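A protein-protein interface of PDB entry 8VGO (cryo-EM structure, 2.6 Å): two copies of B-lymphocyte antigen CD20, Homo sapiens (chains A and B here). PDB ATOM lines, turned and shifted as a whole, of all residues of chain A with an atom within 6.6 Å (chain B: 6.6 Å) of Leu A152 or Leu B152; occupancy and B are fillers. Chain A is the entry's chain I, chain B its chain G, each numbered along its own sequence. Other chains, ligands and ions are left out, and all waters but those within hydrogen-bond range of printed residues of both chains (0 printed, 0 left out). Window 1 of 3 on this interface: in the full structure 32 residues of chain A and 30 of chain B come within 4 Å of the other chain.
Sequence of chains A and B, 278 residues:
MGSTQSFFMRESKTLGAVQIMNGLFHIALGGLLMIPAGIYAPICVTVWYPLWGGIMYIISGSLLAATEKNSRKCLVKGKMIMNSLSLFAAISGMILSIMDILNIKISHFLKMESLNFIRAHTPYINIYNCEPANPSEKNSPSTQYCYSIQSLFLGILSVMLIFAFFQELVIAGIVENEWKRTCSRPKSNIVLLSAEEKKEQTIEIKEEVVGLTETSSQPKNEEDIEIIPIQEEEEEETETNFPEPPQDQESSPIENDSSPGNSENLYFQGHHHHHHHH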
ATOM      1  N   LEU A  32      11.989  29.325  -2.934  1.00  0.00           N
ATOM      2  CA  LEU A  32      11.947  28.133  -3.773  1.00  0.00           C
ATOM      3  C   LEU A  32      13.017  28.172  -4.858  1.00  0.00           C
ATOM      4  O   LEU A  32      13.675  27.162  -5.127  1.00  0.00           O
ATOM      5  CB  LEU A  32      10.557  28.006  -4.391  1.00  0.00           C
ATOM      6  CG  LEU A  32      10.316  26.955  -5.466  1.00  0.00           C
ATOM      7  CD1 LEU A  32      10.613  25.569  -4.931  1.00  0.00           C
ATOM      8  CD2 LEU A  32       8.887  27.060  -5.959  1.00  0.00           C
ATOM      9  N   LEU A  33      13.199  29.327  -5.496  1.00  0.00           N
ATOM     10  CA  LEU A  33      14.223  29.486  -6.522  1.00  0.00           C
ATOM     11  C   LEU A  33      15.633  29.528  -5.940  1.00  0.00           C
ATOM     12  O   LEU A  33      16.601  29.332  -6.680  1.00  0.00           O
ATOM     13  CB  LEU A  33      13.940  30.752  -7.329  1.00  0.00           C
ATOM     14  CG  LEU A  33      14.649  30.980  -8.657  1.00  0.00           C
ATOM     15  CD1 LEU A  33      14.283  29.884  -9.636  1.00  0.00           C
ATOM     16  CD2 LEU A  33      14.257  32.336  -9.206  1.00  0.00           C
ATOM     17  N   ILE A  35      16.449  27.298  -3.667  1.00  0.00           N
ATOM     18  CA  ILE A  35      16.768  25.899  -3.360  1.00  0.00           C
ATOM     19  C   ILE A  35      17.959  25.457  -4.199  1.00  0.00           C
ATOM     20  O   ILE A  35      17.984  25.709  -5.420  1.00  0.00           O
ATOM     21  CB  ILE A  35      15.550  24.997  -3.614  1.00  0.00           C
ATOM     22  CG1 ILE A  35      14.457  25.279  -2.581  1.00  0.00           C
ATOM     23  CG2 ILE A  35      15.947  23.531  -3.595  1.00  0.00           C
ATOM     24  CD1 ILE A  35      13.275  24.348  -2.675  1.00  0.00           C
ATOM     25  N   PRO A  36      18.977  24.820  -3.593  1.00  0.00           N
ATOM     26  CA  PRO A  36      20.188  24.421  -4.324  1.00  0.00           C
ATOM     27  C   PRO A  36      19.934  23.755  -5.666  1.00  0.00           C
ATOM     28  O   PRO A  36      19.219  22.753  -5.760  1.00  0.00           O
ATOM     29  CB  PRO A  36      20.871  23.457  -3.348  1.00  0.00           C
ATOM     30  CG  PRO A  36      20.495  23.985  -2.010  1.00  0.00           C
ATOM     31  CD  PRO A  36      19.080  24.504  -2.159  1.00  0.00           C
ATOM     32  N   ALA A  37      20.523  24.329  -6.715  1.00  0.00           N
ATOM     33  CA  ALA A  37      20.340  23.829  -8.067  1.00  0.00           C
ATOM     34  C   ALA A  37      21.589  23.919  -8.932  1.00  0.00           C
ATOM     35  O   ALA A  37      21.515  23.583 -10.117  1.00  0.00           O
ATOM     36  CB  ALA A  37      19.191  24.569  -8.761  1.00  0.00           C
ATOM     37  N   TYR A 147      17.341  18.304 -17.527  1.00  0.00           N
ATOM     38  CA  TYR A 147      16.270  19.015 -18.222  1.00  0.00           C
ATOM     39  C   TYR A 147      15.037  19.235 -17.353  1.00  0.00           C
ATOM     40  O   TYR A 147      14.287  20.188 -17.587  1.00  0.00           O
ATOM     41  CB  TYR A 147      15.881  18.271 -19.498  1.00  0.00           C
ATOM     42  CG  TYR A 147      16.874  18.432 -20.621  1.00  0.00           C
ATOM     43  CD1 TYR A 147      17.111  19.675 -21.187  1.00  0.00           C
ATOM     44  CD2 TYR A 147      17.563  17.341 -21.130  1.00  0.00           C
ATOM     45  CE1 TYR A 147      18.010  19.831 -22.219  1.00  0.00           C
ATOM     46  CE2 TYR A 147      18.466  17.489 -22.161  1.00  0.00           C
ATOM     47  CZ  TYR A 147      18.686  18.734 -22.702  1.00  0.00           C
ATOM     48  OH  TYR A 147      19.589  18.885 -23.728  1.00  0.00           O
ATOM     49  N   SER A 148      14.799  18.375 -16.363  1.00  0.00           N
ATOM     50  CA  SER A 148      13.722  18.627 -15.410  1.00  0.00           C
ATOM     51  C   SER A 148      13.966  19.887 -14.585  1.00  0.00           C
ATOM     52  O   SER A 148      13.059  20.708 -14.410  1.00  0.00           O
ATOM     53  CB  SER A 148      13.538  17.416 -14.498  1.00  0.00           C
ATOM     54  OG  SER A 148      13.313  16.242 -15.258  1.00  0.00           O
ATOM     55  N   ILE A 149      15.181  20.060 -14.063  1.00  0.00           N
ATOM     56  CA  ILE A 149      15.467  21.249 -13.263  1.00  0.00           C
ATOM     57  C   ILE A 149      15.452  22.507 -14.120  1.00  0.00           C
ATOM     58  O   ILE A 149      14.919  23.546 -13.712  1.00  0.00           O
ATOM     59  CB  ILE A 149      16.815  21.097 -12.538  1.00  0.00           C
ATOM     60  CG1 ILE A 149      16.819  19.855 -11.656  1.00  0.00           C
ATOM     61  CG2 ILE A 149      17.097  22.320 -11.688  1.00  0.00           C
ATOM     62  CD1 ILE A 149      18.190  19.280 -11.435  1.00  0.00           C
ATOM     63  N   GLN A 150      16.038  22.440 -15.315  1.00  0.00           N
ATOM     64  CA  GLN A 150      15.947  23.549 -16.261  1.00  0.00           C
ATOM     65  C   GLN A 150      14.504  23.920 -16.584  1.00  0.00           C
ATOM     66  O   GLN A 150      14.170  25.106 -16.683  1.00  0.00           O
ATOM     67  CB  GLN A 150      16.709  23.198 -17.537  1.00  0.00           C
ATOM     68  CG  GLN A 150      16.827  24.340 -18.522  1.00  0.00           C
ATOM     69  CD  GLN A 150      17.361  23.892 -19.862  1.00  0.00           C
ATOM     70  OE1 GLN A 150      16.600  23.624 -20.790  1.00  0.00           O
ATOM     71  NE2 GLN A 150      18.681  23.806 -19.972  1.00  0.00           N
ATOM     72  N   SER A 151      13.633  22.926 -16.751  1.00  0.00           N
ATOM     73  CA  SER A 151      12.218  23.208 -16.977  1.00  0.00           C
ATOM     74  C   SER A 151      11.532  23.787 -15.743  1.00  0.00           C
ATOM     75  O   SER A 151      10.674  24.667 -15.866  1.00  0.00           O
ATOM     76  CB  SER A 151      11.502  21.941 -17.437  1.00  0.00           C
ATOM     77  OG  SER A 151      12.106  21.412 -18.603  1.00  0.00           O
ATOM     78  N   LEU A 152      11.886  23.308 -14.550  1.00  0.00           N
ATOM     79  CA  LEU A 152      11.349  23.906 -13.329  1.00  0.00           C
ATOM     80  C   LEU A 152      11.781  25.358 -13.155  1.00  0.00           C
ATOM     81  O   LEU A 152      10.967  26.211 -12.788  1.00  0.00           O
ATOM     82  CB  LEU A 152      11.760  23.078 -12.114  1.00  0.00           C
ATOM     83  CG  LEU A 152      10.999  21.764 -11.936  1.00  0.00           C
ATOM     84  CD1 LEU A 152      11.716  20.849 -10.963  1.00  0.00           C
ATOM     85  CD2 LEU A 152       9.584  22.043 -11.466  1.00  0.00           C
ATOM     86  N   PHE A 153      13.053  25.663 -13.412  1.00  0.00           N
ATOM     87  CA  PHE A 153      13.507  27.048 -13.311  1.00  0.00           C
ATOM     88  C   PHE A 153      12.833  27.948 -14.338  1.00  0.00           C
ATOM     89  O   PHE A 153      12.437  29.073 -14.016  1.00  0.00           O
ATOM     90  CB  PHE A 153      15.025  27.116 -13.436  1.00  0.00           C
ATOM     91  CG  PHE A 153      15.726  27.042 -12.119  1.00  0.00           C
ATOM     92  CD1 PHE A 153      15.505  25.982 -11.262  1.00  0.00           C
ATOM     93  CD2 PHE A 153      16.583  28.052 -11.725  1.00  0.00           C
ATOM     94  CE1 PHE A 153      16.138  25.924 -10.042  1.00  0.00           C
ATOM     95  CE2 PHE A 153      17.220  27.996 -10.507  1.00  0.00           C
ATOM     96  CZ  PHE A 153      16.994  26.935  -9.664  1.00  0.00           C
ATOM     97  N   LEU A 154      12.698  27.479 -15.576  1.00  0.00           N
ATOM     98  CA  LEU A 154      11.887  28.200 -16.553  1.00  0.00           C
ATOM     99  C   LEU A 154      10.460  28.403 -16.053  1.00  0.00           C
ATOM    100  O   LEU A 154       9.880  29.481 -16.226  1.00  0.00           O
ATOM    101  CB  LEU A 154      11.893  27.448 -17.883  1.00  0.00           C
ATOM    102  CG  LEU A 154      11.013  27.994 -19.005  1.00  0.00           C
ATOM    103  CD1 LEU A 154      11.519  29.349 -19.465  1.00  0.00           C
ATOM    104  CD2 LEU A 154      10.962  27.016 -20.165  1.00  0.00           C
ATOM    105  N   GLY A 155       9.877  27.374 -15.437  1.00  0.00           N
ATOM    106  CA  GLY A 155       8.555  27.515 -14.844  1.00  0.00           C
ATOM    107  C   GLY A 155       8.482  28.537 -13.724  1.00  0.00           C
ATOM    108  O   GLY A 155       7.610  29.409 -13.721  1.00  0.00           O
ATOM    109  N   ILE A 156       9.391  28.440 -12.751  1.00  0.00           N
ATOM    110  CA  ILE A 156       9.405  29.386 -11.634  1.00  0.00           C
ATOM    111  C   ILE A 156       9.623  30.816 -12.114  1.00  0.00           C
ATOM    112  O   ILE A 156       8.972  31.751 -11.632  1.00  0.00           O
ATOM    113  CB  ILE A 156      10.473  28.981 -10.602  1.00  0.00           C
ATOM    114  CG1 ILE A 156      10.154  27.615  -9.998  1.00  0.00           C
ATOM    115  CG2 ILE A 156      10.575  30.020  -9.504  1.00  0.00           C
ATOM    116  CD1 ILE A 156      11.362  26.900  -9.449  1.00  0.00           C
ATOM    117  N   LEU A 157      10.526  31.013 -13.074  1.00  0.00           N
ATOM    118  CA  LEU A 157      10.803  32.362 -13.557  1.00  0.00           C
ATOM    119  C   LEU A 157       9.616  32.952 -14.312  1.00  0.00           C
ATOM    120  O   LEU A 157       9.291  34.131 -14.135  1.00  0.00           O
ATOM    121  CB  LEU A 157      12.052  32.355 -14.434  1.00  0.00           C
ATOM    122  CG  LEU A 157      13.352  32.099 -13.672  1.00  0.00           C
ATOM    123  CD1 LEU A 157      14.473  31.729 -14.623  1.00  0.00           C
ATOM    124  CD2 LEU A 157      13.727  33.313 -12.844  1.00  0.00           C
ATOM    125  N   LEU B  32       3.303  24.668 -12.183  1.00  0.00           N
ATOM    126  CA  LEU B  32       4.721  24.453 -11.923  1.00  0.00           C
ATOM    127  C   LEU B  32       4.987  23.046 -11.404  1.00  0.00           C
ATOM    128  O   LEU B  32       5.950  22.392 -11.818  1.00  0.00           O
ATOM    129  CB  LEU B  32       5.213  25.499 -10.927  1.00  0.00           C
ATOM    130  CG  LEU B  32       6.609  25.358 -10.335  1.00  0.00           C
ATOM    131  CD1 LEU B  32       7.654  25.367 -11.432  1.00  0.00           C
ATOM    132  CD2 LEU B  32       6.849  26.476  -9.340  1.00  0.00           C
ATOM    133  N   LEU B  33       4.147  22.565 -10.488  1.00  0.00           N
ATOM    134  CA  LEU B  33       4.280  21.215  -9.956  1.00  0.00           C
ATOM    135  C   LEU B  33       3.875  20.145 -10.964  1.00  0.00           C
ATOM    136  O   LEU B  33       4.234  18.977 -10.787  1.00  0.00           O
ATOM    137  CB  LEU B  33       3.449  21.089  -8.680  1.00  0.00           C
ATOM    138  CG  LEU B  33       3.670  19.910  -7.742  1.00  0.00           C
ATOM    139  CD1 LEU B  33       5.087  19.926  -7.210  1.00  0.00           C
ATOM    140  CD2 LEU B  33       2.674  19.983  -6.605  1.00  0.00           C
ATOM    141  N   ILE B  35       4.979  20.412 -14.051  1.00  0.00           N
ATOM    142  CA  ILE B  35       6.116  20.320 -14.975  1.00  0.00           C
ATOM    143  C   ILE B  35       6.717  18.923 -14.894  1.00  0.00           C
ATOM    144  O   ILE B  35       6.944  18.410 -13.780  1.00  0.00           O
ATOM    145  CB  ILE B  35       7.168  21.394 -14.649  1.00  0.00           C
ATOM    146  CG1 ILE B  35       6.627  22.784 -14.986  1.00  0.00           C
ATOM    147  CG2 ILE B  35       8.465  21.122 -15.389  1.00  0.00           C
ATOM    148  CD1 ILE B  35       7.638  23.888 -14.813  1.00  0.00           C
ATOM    149  N   PRO B  36       6.970  18.261 -16.036  1.00  0.00           N
ATOM    150  CA  PRO B  36       7.491  16.887 -16.035  1.00  0.00           C
ATOM    151  C   PRO B  36       8.639  16.643 -15.072  1.00  0.00           C
ATOM    152  O   PRO B  36       9.668  17.322 -15.112  1.00  0.00           O
ATOM    153  CB  PRO B  36       7.937  16.693 -17.490  1.00  0.00           C
ATOM    154  CG  PRO B  36       6.983  17.527 -18.266  1.00  0.00           C
ATOM    155  CD  PRO B  36       6.706  18.742 -17.403  1.00  0.00           C
ATOM    156  N   ALA B  37       8.448  15.662 -14.188  1.00  0.00           N
ATOM    157  CA  ALA B  37       9.439  15.338 -13.176  1.00  0.00           C
ATOM    158  C   ALA B  37       9.556  13.848 -12.885  1.00  0.00           C
ATOM    159  O   ALA B  37      10.320  13.477 -11.990  1.00  0.00           O
ATOM    160  CB  ALA B  37       9.137  16.084 -11.872  1.00  0.00           C
ATOM    161  N   TYR B 147      18.412  14.693  -6.262  1.00  0.00           N
ATOM    162  CA  TYR B 147      18.134  15.368  -4.997  1.00  0.00           C
ATOM    163  C   TYR B 147      17.732  16.828  -5.172  1.00  0.00           C
ATOM    164  O   TYR B 147      17.023  17.374  -4.321  1.00  0.00           O
ATOM    165  CB  TYR B 147      19.343  15.272  -4.069  1.00  0.00           C
ATOM    166  CG  TYR B 147      19.519  13.913  -3.439  1.00  0.00           C
ATOM    167  CD1 TYR B 147      18.566  13.405  -2.569  1.00  0.00           C
ATOM    168  CD2 TYR B 147      20.641  13.144  -3.699  1.00  0.00           C
ATOM    169  CE1 TYR B 147      18.720  12.167  -1.984  1.00  0.00           C
ATOM    170  CE2 TYR B 147      20.803  11.903  -3.118  1.00  0.00           C
ATOM    171  CZ  TYR B 147      19.841  11.421  -2.262  1.00  0.00           C
ATOM    172  OH  TYR B 147      19.997  10.181  -1.685  1.00  0.00           O
ATOM    173  N   SER B 148      18.168  17.479  -6.249  1.00  0.00           N
ATOM    174  CA  SER B 148      17.686  18.827  -6.543  1.00  0.00           C
ATOM    175  C   SER B 148      16.189  18.852  -6.835  1.00  0.00           C
ATOM    176  O   SER B 148      15.463  19.706  -6.316  1.00  0.00           O
ATOM    177  CB  SER B 148      18.472  19.420  -7.711  1.00  0.00           C
ATOM    178  OG  SER B 148      19.862  19.399  -7.446  1.00  0.00           O
ATOM    179  N   ILE B 149      15.704  17.928  -7.666  1.00  0.00           N
ATOM    180  CA  ILE B 149      14.278  17.910  -7.983  1.00  0.00           C
ATOM    181  C   ILE B 149      13.449  17.517  -6.767  1.00  0.00           C
ATOM    182  O   ILE B 149      12.394  18.105  -6.503  1.00  0.00           O
ATOM    183  CB  ILE B 149      14.002  16.962  -9.162  1.00  0.00           C
ATOM    184  CG1 ILE B 149      14.806  17.375 -10.387  1.00  0.00           C
ATOM    185  CG2 ILE B 149      12.525  16.964  -9.505  1.00  0.00           C
ATOM    186  CD1 ILE B 149      15.110  16.236 -11.319  1.00  0.00           C
ATOM    187  N   GLN B 150      13.904  16.517  -6.012  1.00  0.00           N
ATOM    188  CA  GLN B 150      13.254  16.169  -4.753  1.00  0.00           C
ATOM    189  C   GLN B 150      13.187  17.348  -3.789  1.00  0.00           C
ATOM    190  O   GLN B 150      12.170  17.549  -3.115  1.00  0.00           O
ATOM    191  CB  GLN B 150      13.981  14.991  -4.108  1.00  0.00           C
ATOM    192  CG  GLN B 150      13.294  14.434  -2.881  1.00  0.00           C
ATOM    193  CD  GLN B 150      14.159  13.444  -2.136  1.00  0.00           C
ATOM    194  OE1 GLN B 150      14.837  13.797  -1.174  1.00  0.00           O
ATOM    195  NE2 GLN B 150      14.139  12.194  -2.579  1.00  0.00           N
ATOM    196  N   SER B 151      14.255  18.141  -3.706  1.00  0.00           N
ATOM    197  CA  SER B 151      14.230  19.336  -2.867  1.00  0.00           C
ATOM    198  C   SER B 151      13.302  20.416  -3.416  1.00  0.00           C
ATOM    199  O   SER B 151      12.631  21.109  -2.642  1.00  0.00           O
ATOM    200  CB  SER B 151      15.645  19.886  -2.703  1.00  0.00           C
ATOM    201  OG  SER B 151      16.510  18.905  -2.161  1.00  0.00           O
ATOM    202  N   LEU B 152      13.250  20.585  -4.738  1.00  0.00           N
ATOM    203  CA  LEU B 152      12.293  21.520  -5.323  1.00  0.00           C
ATOM    204  C   LEU B 152      10.847  21.108  -5.067  1.00  0.00           C
ATOM    205  O   LEU B 152      10.010  21.953  -4.730  1.00  0.00           O
ATOM    206  CB  LEU B 152      12.549  21.662  -6.823  1.00  0.00           C
ATOM    207  CG  LEU B 152      13.768  22.504  -7.197  1.00  0.00           C
ATOM    208  CD1 LEU B 152      14.163  22.276  -8.643  1.00  0.00           C
ATOM    209  CD2 LEU B 152      13.483  23.972  -6.944  1.00  0.00           C
ATOM    210  N   PHE B 153      10.531  19.823  -5.214  1.00  0.00           N
ATOM    211  CA  PHE B 153       9.172  19.368  -4.930  1.00  0.00           C
ATOM    212  C   PHE B 153       8.806  19.536  -3.462  1.00  0.00           C
ATOM    213  O   PHE B 153       7.692  19.962  -3.141  1.00  0.00           O
ATOM    214  CB  PHE B 153       8.997  17.920  -5.377  1.00  0.00           C
ATOM    215  CG  PHE B 153       8.489  17.795  -6.774  1.00  0.00           C
ATOM    216  CD1 PHE B 153       9.160  18.393  -7.824  1.00  0.00           C
ATOM    217  CD2 PHE B 153       7.322  17.104  -7.038  1.00  0.00           C
ATOM    218  CE1 PHE B 153       8.683  18.291  -9.110  1.00  0.00           C
ATOM    219  CE2 PHE B 153       6.843  16.998  -8.322  1.00  0.00           C
ATOM    220  CZ  PHE B 153       7.520  17.595  -9.358  1.00  0.00           C
ATOM    221  N   LEU B 154       9.723  19.203  -2.555  1.00  0.00           N
ATOM    222  CA  LEU B 154       9.517  19.526  -1.147  1.00  0.00           C
ATOM    223  C   LEU B 154       9.291  21.022  -0.945  1.00  0.00           C
ATOM    224  O   LEU B 154       8.428  21.427  -0.158  1.00  0.00           O
ATOM    225  CB  LEU B 154      10.712  19.043  -0.328  1.00  0.00           C
ATOM    226  CG  LEU B 154      10.730  19.384   1.162  1.00  0.00           C
ATOM    227  CD1 LEU B 154       9.607  18.666   1.884  1.00  0.00           C
ATOM    228  CD2 LEU B 154      12.075  19.032   1.771  1.00  0.00           C
ATOM    229  N   GLY B 155      10.064  21.854  -1.642  1.00  0.00           N
ATOM    230  CA  GLY B 155       9.849  23.294  -1.582  1.00  0.00           C
ATOM    231  C   GLY B 155       8.492  23.742  -2.097  1.00  0.00           C
ATOM    232  O   GLY B 155       7.782  24.497  -1.429  1.00  0.00           O
ATOM    233  N   ILE B 156       8.115  23.291  -3.296  1.00  0.00           N
ATOM    234  CA  ILE B 156       6.820  23.661  -3.869  1.00  0.00           C
ATOM    235  C   ILE B 156       5.665  23.194  -2.991  1.00  0.00           C
ATOM    236  O   ILE B 156       4.692  23.929  -2.784  1.00  0.00           O
ATOM    237  CB  ILE B 156       6.688  23.103  -5.298  1.00  0.00           C
ATOM    238  CG1 ILE B 156       7.746  23.708  -6.218  1.00  0.00           C
ATOM    239  CG2 ILE B 156       5.304  23.376  -5.852  1.00  0.00           C
ATOM    240  CD1 ILE B 156       8.070  22.850  -7.414  1.00  0.00           C
ATOM    241  N   LEU B 157       5.753  21.979  -2.452  1.00  0.00           N
ATOM    242  CA  LEU B 157       4.666  21.462  -1.625  1.00  0.00           C
ATOM    243  C   LEU B 157       4.537  22.225  -0.311  1.00  0.00           C
ATOM    244  O   LEU B 157       3.420  22.528   0.124  1.00  0.00           O
ATOM    245  CB  LEU B 157       4.874  19.972  -1.368  1.00  0.00           C
ATOM    246  CG  LEU B 157       4.682  19.090  -2.600  1.00  0.00           C
ATOM    247  CD1 LEU B 157       5.266  17.709  -2.374  1.00  0.00           C
ATOM    248  CD2 LEU B 157       3.212  19.001  -2.962  1.00  0.00           C
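O of Tyr B147 lies within hydrogen-bond range of OG of Ser B151 (2.7 Å). The backbone carbonyl oxygen (O) of Tyr A147 is in hydrogen-bond range of the side-chain hydroxyl (OG) of Ser A151 (2.7 Å).
Hydrophobic or aromatic side chains of chain B that line the printed part of chain A: Leu B32, Ile B35, Ile B149, Leu B152 and Ile B156. Along chain B the printed residues that touch a printed residue of chain A span positions 32 to 156. Printed residues of chain A that touch a printed residue of chain B: Leu A32, Ile A35, Pro A36, Ser A148, Ile A149, Ser A151, Leu A152, Gly A155 and Ile A156. Hydrophobic or aromatic side chains of chain A within 4 Å of the printed part of chain B: Leu A32, Ile A35, Ile A149, Leu A152 and Ile A156. Among the printed residues, 19 pairs touch across the chains. Among the printed residues, no Asp or Glu carboxylate lies within 4 Å of a Lys or Arg side-chain nitrogen of the other chain.
Among the printed residues, pairs that only touch across the chains: Leu A32 with Leu B32 (3.99 Å), Leu A32 with Leu B152 (3.7 Å), Leu A32 with Gly B155 (3.98 Å), Leu A32 with Ile B156 (3.6 Å), Ile A35 with Ser B151 (3.3 Å), Ile A35 with Leu B152 (3.997 Å), Ile A35 with Gly B155 (3.7 Å), Pro A36 with Ser B148 (3.8 Å), Ser A148 with Pro B36 (3.8 Å), Ser A148 with Ile B149 (3.7 Å), Ile A149 with Ser B148 (3.7 Å), Ile A149 with Ile B149 (3.4 Å), Ser A151 with Ile B35 (3.3 Å), Leu A152 with Leu B32 (3.7 Å), Leu A152 with Ile B35 (3.997 Å), Leu A152 with Leu B152 (3.7 Å), Gly A155 with Leu B32 (3.998 Å), Gly A155 with Ile B35 (3.7 Å) and Ile A156 with Leu B32 (3.6 Å).
Ile A35 touches Ser B151, and with the chains exchanged Ser A151 touches Ile B35. Ile A35 touches Leu B152, and with the chains exchanged Leu A152 touches Ile B35. Ile A35 touches Gly B155, and with the chains exchanged Gly A155 touches Ile B35. Pro A36 touches Ser B148, and with the chains exchanged Ser A148 touches Pro B36. Positions printed for both chains: 32, 33, 35, 36, 37, 147, 148, 149, 150, 151, 152, 153, 154, 155, 156 and 157.
Of the printed residues of chain B, Leu A152 touches Leu B32, Ile B35 and Leu B152. Of the printed residues of chain A, Leu B152 touches Leu A32, Ile A35 and Leu A152. Printed residues of chain A within 4 Å of Leu B32: Leu A32, Leu A152, Gly A155 and Ile A156. Of the printed residues of chain B, Leu A32 touches Leu B32 (3.99 Å), Leu B152 (3.7 Å), Gly B155 (3.98 Å) and Ile B156 (3.6 Å). Printed residues of chain B within 4 Å of Ser A151: Ile B35. Printed residues of chain B within 4 Å of Ile A35: Ser B151, Leu B152 and Gly B155. Of the printed residues of chain A, Ser B151 touches Ile A35. Leu A154 touches none of the printed residues of chain B. The nearest printed residue of chain A that does not touch Leu B152 is Ile A149 (4.2 Å).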
